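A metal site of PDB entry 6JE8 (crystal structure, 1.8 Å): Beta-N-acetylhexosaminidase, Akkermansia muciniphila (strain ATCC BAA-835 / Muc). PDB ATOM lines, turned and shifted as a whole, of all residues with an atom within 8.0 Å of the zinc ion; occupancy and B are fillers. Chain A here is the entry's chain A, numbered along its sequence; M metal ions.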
ATOM      1  N   PHE A 204      19.324 -11.327  -3.502  1.00  0.00           N
ATOM      2  CA  PHE A 204      20.282 -11.399  -2.407  1.00  0.00           C
ATOM      3  C   PHE A 204      21.356 -12.467  -2.613  1.00  0.00           C
ATOM      4  O   PHE A 204      22.261 -12.580  -1.779  1.00  0.00           O
ATOM      5  CB  PHE A 204      19.588 -11.696  -1.071  1.00  0.00           C
ATOM      6  CG  PHE A 204      18.666 -10.595  -0.577  1.00  0.00           C
ATOM      7  CD1 PHE A 204      18.543  -9.389  -1.245  1.00  0.00           C
ATOM      8  CD2 PHE A 204      17.906 -10.808   0.574  1.00  0.00           C
ATOM      9  CE1 PHE A 204      17.681  -8.388  -0.760  1.00  0.00           C
ATOM     10  CE2 PHE A 204      17.049  -9.826   1.062  1.00  0.00           C
ATOM     11  CZ  PHE A 204      16.934  -8.617   0.399  1.00  0.00           C
ATOM     12  N   PHE A 205      21.254 -13.281  -3.671  1.00  0.00           N
ATOM     13  CA  PHE A 205      22.043 -14.500  -3.788  1.00  0.00           C
ATOM     14  C   PHE A 205      22.976 -14.438  -4.995  1.00  0.00           C
ATOM     15  O   PHE A 205      22.739 -13.672  -5.929  1.00  0.00           O
ATOM     16  CB  PHE A 205      21.118 -15.727  -3.881  1.00  0.00           C
ATOM     17  CG  PHE A 205      20.343 -15.943  -2.609  1.00  0.00           C
ATOM     18  CD1 PHE A 205      19.226 -15.151  -2.337  1.00  0.00           C
ATOM     19  CD2 PHE A 205      20.790 -16.845  -1.659  1.00  0.00           C
ATOM     20  CE1 PHE A 205      18.540 -15.280  -1.139  1.00  0.00           C
ATOM     21  CE2 PHE A 205      20.085 -17.010  -0.448  1.00  0.00           C
ATOM     22  CZ  PHE A 205      18.949 -16.227  -0.201  1.00  0.00           C
ATOM     23  N   CYS A 206      24.050 -15.246  -4.937  1.00  0.00           N
ATOM     24  CA  CYS A 206      25.052 -15.233  -6.004  1.00  0.00           C
ATOM     25  C   CYS A 206      24.432 -15.563  -7.347  1.00  0.00           C
ATOM     26  O   CYS A 206      24.761 -14.934  -8.368  1.00  0.00           O
ATOM     27  CB  CYS A 206      26.179 -16.224  -5.698  1.00  0.00           C
ATOM     28  SG  CYS A 206      26.997 -15.940  -4.108  1.00  0.00           S
ATOM     29  N   PHE A 207      23.528 -16.540  -7.377  1.00  0.00           N
ATOM     30  CA  PHE A 207      22.865 -16.978  -8.605  1.00  0.00           C
ATOM     31  C   PHE A 207      21.363 -16.882  -8.408  1.00  0.00           C
ATOM     32  O   PHE A 207      20.701 -17.875  -8.044  1.00  0.00           O
ATOM     33  CB  PHE A 207      23.305 -18.396  -8.972  1.00  0.00           C
ATOM     34  CG  PHE A 207      24.761 -18.474  -9.282  1.00  0.00           C
ATOM     35  CD1 PHE A 207      25.229 -18.166 -10.549  1.00  0.00           C
ATOM     36  CD2 PHE A 207      25.674 -18.786  -8.278  1.00  0.00           C
ATOM     37  CE1 PHE A 207      26.580 -18.216 -10.832  1.00  0.00           C
ATOM     38  CE2 PHE A 207      27.032 -18.833  -8.556  1.00  0.00           C
ATOM     39  CZ  PHE A 207      27.490 -18.551  -9.829  1.00  0.00           C
ATOM     40  N   LEU A 224      23.412 -19.601  -0.660  1.00  0.00           N
ATOM     41  CA  LEU A 224      23.959 -18.691   0.330  1.00  0.00           C
ATOM     42  C   LEU A 224      23.776 -17.254  -0.137  1.00  0.00           C
ATOM     43  O   LEU A 224      23.947 -16.965  -1.323  1.00  0.00           O
ATOM     44  CB  LEU A 224      25.454 -18.944   0.556  1.00  0.00           C
ATOM     45  CG  LEU A 224      25.894 -20.382   0.784  1.00  0.00           C
ATOM     46  CD1 LEU A 224      27.407 -20.401   1.047  1.00  0.00           C
ATOM     47  CD2 LEU A 224      25.119 -20.990   1.935  1.00  0.00           C
ATOM     48  N   VAL A 225      23.471 -16.336   0.802  1.00  0.00           N
ATOM     49  CA  VAL A 225      23.450 -14.932   0.416  1.00  0.00           C
ATOM     50  C   VAL A 225      24.838 -14.523  -0.078  1.00  0.00           C
ATOM     51  O   VAL A 225      25.858 -15.079   0.351  1.00  0.00           O
ATOM     52  CB  VAL A 225      22.989 -14.003   1.552  1.00  0.00           C
ATOM     53  CG1 VAL A 225      21.518 -14.258   1.863  1.00  0.00           C
ATOM     54  CG2 VAL A 225      23.850 -14.222   2.810  1.00  0.00           C
ATOM     55  N   CYS A 226      24.869 -13.575  -1.016  1.00  0.00           N
ATOM     56  CA  CYS A 226      26.132 -13.132  -1.591  1.00  0.00           C
ATOM     57  C   CYS A 226      26.666 -11.972  -0.775  1.00  0.00           C
ATOM     58  O   CYS A 226      26.043 -10.894  -0.766  1.00  0.00           O
ATOM     59  CB  CYS A 226      25.958 -12.721  -3.058  1.00  0.00           C
ATOM     60  SG  CYS A 226      27.530 -12.098  -3.777  1.00  0.00           S
ATOM     61  N   PRO A 227      27.797 -12.128  -0.069  1.00  0.00           N
ATOM     62  CA  PRO A 227      28.307 -11.060   0.802  1.00  0.00           C
ATOM     63  C   PRO A 227      28.767  -9.828   0.035  1.00  0.00           C
ATOM     64  O   PRO A 227      29.036  -8.797   0.679  1.00  0.00           O
ATOM     65  CB  PRO A 227      29.491 -11.727   1.515  1.00  0.00           C
ATOM     66  CG  PRO A 227      29.317 -13.174   1.335  1.00  0.00           C
ATOM     67  CD  PRO A 227      28.594 -13.366   0.045  1.00  0.00           C
ATOM     68  N   GLN A 228      28.874  -9.901  -1.289  1.00  0.00           N
ATOM     69  CA  GLN A 228      29.267  -8.743  -2.064  1.00  0.00           C
ATOM     70  C   GLN A 228      28.122  -7.800  -2.369  1.00  0.00           C
ATOM     71  O   GLN A 228      28.355  -6.726  -2.939  1.00  0.00           O
ATOM     72  CB  GLN A 228      29.902  -9.171  -3.394  1.00  0.00           C
ATOM     73  CG  GLN A 228      30.828 -10.382  -3.339  1.00  0.00           C
ATOM     74  CD  GLN A 228      31.762 -10.353  -2.117  1.00  0.00           C
ATOM     75  OE1 GLN A 228      32.212  -9.298  -1.689  1.00  0.00           O
ATOM     76  NE2 GLN A 228      32.044 -11.536  -1.572  1.00  0.00           N
ATOM     77  N   LYS A 229      26.893  -8.160  -2.034  1.00  0.00           N
ATOM     78  CA  LYS A 229      25.748  -7.378  -2.472  1.00  0.00           C
ATOM     79  C   LYS A 229      25.276  -6.455  -1.354  1.00  0.00           C
ATOM     80  O   LYS A 229      24.963  -6.948  -0.250  1.00  0.00           O
ATOM     81  CB  LYS A 229      24.621  -8.297  -2.932  1.00  0.00           C
ATOM     82  CG  LYS A 229      24.990  -9.025  -4.209  1.00  0.00           C
ATOM     83  CD  LYS A 229      23.858  -9.843  -4.803  1.00  0.00           C
ATOM     84  CE  LYS A 229      24.267 -10.397  -6.173  1.00  0.00           C
ATOM     85  NZ  LYS A 229      23.188 -11.202  -6.839  1.00  0.00           N
ATOM     86  N   LEU A 263      28.528 -22.468  -4.372  1.00  0.00           N
ATOM     87  CA  LEU A 263      28.043 -21.322  -5.143  1.00  0.00           C
ATOM     88  C   LEU A 263      28.891 -20.077  -4.886  1.00  0.00           C
ATOM     89  O   LEU A 263      29.121 -19.278  -5.804  1.00  0.00           O
ATOM     90  CB  LEU A 263      26.567 -21.052  -4.845  1.00  0.00           C
ATOM     91  CG  LEU A 263      25.618 -22.159  -5.345  1.00  0.00           C
ATOM     92  CD1 LEU A 263      24.158 -21.687  -5.238  1.00  0.00           C
ATOM     93  CD2 LEU A 263      25.957 -22.606  -6.772  1.00  0.00           C
ATOM     94  N   TRP A 264      29.393 -19.897  -3.655  1.00  0.00           N
ATOM     95  CA  TRP A 264      30.367 -18.834  -3.437  1.00  0.00           C
ATOM     96  C   TRP A 264      31.612 -19.049  -4.289  1.00  0.00           C
ATOM     97  O   TRP A 264      32.195 -18.095  -4.799  1.00  0.00           O
ATOM     98  CB  TRP A 264      30.790 -18.771  -1.973  1.00  0.00           C
ATOM     99  CG  TRP A 264      29.860 -18.015  -1.093  1.00  0.00           C
ATOM    100  CD1 TRP A 264      28.636 -17.481  -1.428  1.00  0.00           C
ATOM    101  CD2 TRP A 264      30.079 -17.702   0.277  1.00  0.00           C
ATOM    102  NE1 TRP A 264      28.090 -16.847  -0.324  1.00  0.00           N
ATOM    103  CE2 TRP A 264      28.955 -16.973   0.734  1.00  0.00           C
ATOM    104  CE3 TRP A 264      31.115 -17.976   1.183  1.00  0.00           C
ATOM    105  CZ2 TRP A 264      28.845 -16.515   2.034  1.00  0.00           C
ATOM    106  CZ3 TRP A 264      31.015 -17.505   2.478  1.00  0.00           C
ATOM    107  CH2 TRP A 264      29.879 -16.785   2.903  1.00  0.00           C
ATOM    108  N   GLU A 265      32.048 -20.310  -4.419  1.00  0.00           N
ATOM    109  CA  GLU A 265      33.243 -20.573  -5.221  1.00  0.00           C
ATOM    110  C   GLU A 265      33.038 -20.134  -6.660  1.00  0.00           C
ATOM    111  O   GLU A 265      33.938 -19.527  -7.265  1.00  0.00           O
ATOM    112  CB  GLU A 265      33.610 -22.062  -5.159  1.00  0.00           C
ATOM    113  CG  GLU A 265      34.959 -22.400  -5.802  1.00  0.00           C
ATOM    114  CD  GLU A 265      34.894 -22.484  -7.320  1.00  0.00           C
ATOM    115  OE1 GLU A 265      33.907 -23.016  -7.853  1.00  0.00           O
ATOM    116  OE2 GLU A 265      35.836 -21.982  -7.982  1.00  0.00           O
ATOM    117  N   LYS A 266      31.838 -20.393  -7.210  1.00  0.00           N
ATOM    118  CA  LYS A 266      31.533 -20.081  -8.608  1.00  0.00           C
ATOM    119  C   LYS A 266      31.138 -18.621  -8.842  1.00  0.00           C
ATOM    120  O   LYS A 266      31.243 -18.143  -9.986  1.00  0.00           O
ATOM    121  CB  LYS A 266      30.402 -20.965  -9.105  1.00  0.00           C
ATOM    122  CG  LYS A 266      30.768 -22.426  -9.175  1.00  0.00           C
ATOM    123  CD  LYS A 266      29.652 -23.263  -9.782  1.00  0.00           C
ATOM    124  CE  LYS A 266      30.079 -24.726  -9.848  1.00  0.00           C
ATOM    125  NZ  LYS A 266      28.947 -25.642 -10.168  1.00  0.00           N
ATOM    126  N   CYS A 267      30.656 -17.910  -7.828  1.00  0.00           N
ATOM    127  CA  CYS A 267      30.141 -16.549  -8.010  1.00  0.00           C
ATOM    128  C   CYS A 267      31.180 -15.603  -8.595  1.00  0.00           C
ATOM    129  O   CYS A 267      32.255 -15.437  -8.007  1.00  0.00           O
ATOM    130  CB  CYS A 267      29.660 -16.000  -6.662  1.00  0.00           C
ATOM    131  SG  CYS A 267      29.085 -14.288  -6.738  1.00  0.00           S
ATOM    132  N   PRO A 268      30.903 -14.914  -9.710  1.00  0.00           N
ATOM    133  CA  PRO A 268      31.925 -13.987 -10.259  1.00  0.00           C
ATOM    134  C   PRO A 268      32.236 -12.819  -9.337  1.00  0.00           C
ATOM    135  O   PRO A 268      33.396 -12.365  -9.275  1.00  0.00           O
ATOM    136  CB  PRO A 268      31.300 -13.523 -11.589  1.00  0.00           C
ATOM    137  CG  PRO A 268      29.804 -13.797 -11.461  1.00  0.00           C
ATOM    138  CD  PRO A 268      29.690 -15.006 -10.542  1.00  0.00           C
ATOM    139  N   LEU A 269      31.237 -12.345  -8.563  1.00  0.00           N
ATOM    140  CA  LEU A 269      31.485 -11.292  -7.587  1.00  0.00           C
ATOM    141  C   LEU A 269      32.366 -11.801  -6.449  1.00  0.00           C
ATOM    142  O   LEU A 269      33.340 -11.152  -6.067  1.00  0.00           O
ATOM    143  CB  LEU A 269      30.164 -10.748  -7.020  1.00  0.00           C
ATOM    144  CG  LEU A 269      29.128 -10.206  -8.019  1.00  0.00           C
ATOM    145  CD1 LEU A 269      27.884  -9.734  -7.273  1.00  0.00           C
ATOM    146  CD2 LEU A 269      29.731  -9.065  -8.814  1.00  0.00           C
ATOM    147  N   CYS A 270      31.998 -12.956  -5.872  1.00  0.00           N
ATOM    148  CA  CYS A 270      32.787 -13.488  -4.771  1.00  0.00           C
ATOM    149  C   CYS A 270      34.193 -13.869  -5.222  1.00  0.00           C
ATOM    150  O   CYS A 270      35.154 -13.716  -4.469  1.00  0.00           O
ATOM    151  CB  CYS A 270      32.077 -14.690  -4.141  1.00  0.00           C
ATOM    152  SG  CYS A 270      30.577 -14.217  -3.214  1.00  0.00           S
ATOM    153  N   ARG A 271      34.333 -14.400  -6.444  1.00  0.00           N
ATOM    154  CA  ARG A 271      35.670 -14.744  -6.928  1.00  0.00           C
ATOM    155  C   ARG A 271      36.574 -13.536  -6.908  1.00  0.00           C
ATOM    156  O   ARG A 271      37.697 -13.575  -6.362  1.00  0.00           O
ATOM    157  CB  ARG A 271      35.595 -15.318  -8.337  1.00  0.00           C
ATOM    158  CG  ARG A 271      35.143 -16.749  -8.387  1.00  0.00           C
ATOM    159  CD  ARG A 271      35.059 -17.212  -9.813  1.00  0.00           C
ATOM    160  NE  ARG A 271      34.893 -18.656  -9.870  1.00  0.00           N
ATOM    161  CZ  ARG A 271      34.780 -19.338 -10.994  1.00  0.00           C
ATOM    162  NH1 ARG A 271      34.824 -18.702 -12.164  1.00  0.00           N
ATOM    163  NH2 ARG A 271      34.621 -20.655 -10.950  1.00  0.00           N
ATOM    164  N   ALA A 273      36.137 -10.728  -5.246  1.00  0.00           N
ATOM    165  CA  ALA A 273      36.314 -10.248  -3.878  1.00  0.00           C
ATOM    166  C   ALA A 273      37.392 -11.036  -3.139  1.00  0.00           C
ATOM    167  O   ALA A 273      38.197 -10.446  -2.401  1.00  0.00           O
ATOM    168  CB  ALA A 273      34.982 -10.337  -3.108  1.00  0.00           C
ATOM    169  N   ARG A 274      37.399 -12.362  -3.285  1.00  0.00           N
ATOM    170  CA  ARG A 274      38.430 -13.170  -2.636  1.00  0.00           C
ATOM    171  C   ARG A 274      39.808 -12.824  -3.172  1.00  0.00           C
ATOM    172  O   ARG A 274      40.781 -12.773  -2.412  1.00  0.00           O
ATOM    173  CB  ARG A 274      38.150 -14.662  -2.837  1.00  0.00           C
ATOM    174  CG  ARG A 274      37.012 -15.220  -1.993  1.00  0.00           C
ATOM    175  CD  ARG A 274      37.011 -16.757  -2.014  1.00  0.00           C
ATOM    176  NE  ARG A 274      36.950 -17.328  -3.366  1.00  0.00           N
ATOM    177  CZ  ARG A 274      35.833 -17.514  -4.053  1.00  0.00           C
ATOM    178  NH1 ARG A 274      34.646 -17.174  -3.544  1.00  0.00           N
ATOM    179  NH2 ARG A 274      35.893 -18.045  -5.268  1.00  0.00           N
ATOM    180  N   GLN A 285      36.460 -16.712   3.297  1.00  0.00           N
ATOM    181  CA  GLN A 285      35.326 -15.845   3.022  1.00  0.00           C
ATOM    182  C   GLN A 285      34.253 -15.981   4.102  1.00  0.00           C
ATOM    183  O   GLN A 285      33.659 -14.978   4.522  1.00  0.00           O
ATOM    184  CB  GLN A 285      34.746 -16.158   1.646  1.00  0.00           C
ATOM    185  CG  GLN A 285      33.733 -15.141   1.188  1.00  0.00           C
ATOM    186  CD  GLN A 285      33.164 -15.480  -0.170  1.00  0.00           C
ATOM    187  OE1 GLN A 285      33.770 -16.236  -0.938  1.00  0.00           O
ATOM    188  NE2 GLN A 285      31.988 -14.944  -0.462  1.00  0.00           N
HETATM  189 ZN    ZN M   1      28.514 -14.113  -4.451  1.00  0.00          ZN
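The side-chain sulfur (SG) of Cys 226 sits close to the backbone NH (N) of Gln 228.
The backbone NH of Cys 226 is in hydrogen-bond range of the backbone carbonyl oxygen of Phe 204, 2.9 Å away.
The side-chain sulfur (SG) of Cys 267 lies close to the backbone NH (N) of Leu 269 (3.4 Å).
The side-chain amide nitrogen (NE2) of Gln 228 lies close to the side-chain sulfur (SG) of Cys 270, 3.5 Å away.
NE2 of Gln 285 lies close to SG of Cys 270 (3.2 Å).
The nearest printed residue that does not touch the zinc ion is Trp 264 (4.5 Å).
The zinc ion is bound by SG of Cys 226 (2.3 Å), SG of Cys 267 (2.4 Å), SG of Cys 206 (2.4 Å) and SG of Cys 270 (2.4 Å).
The zinc ion has four donor atoms within binding distance.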
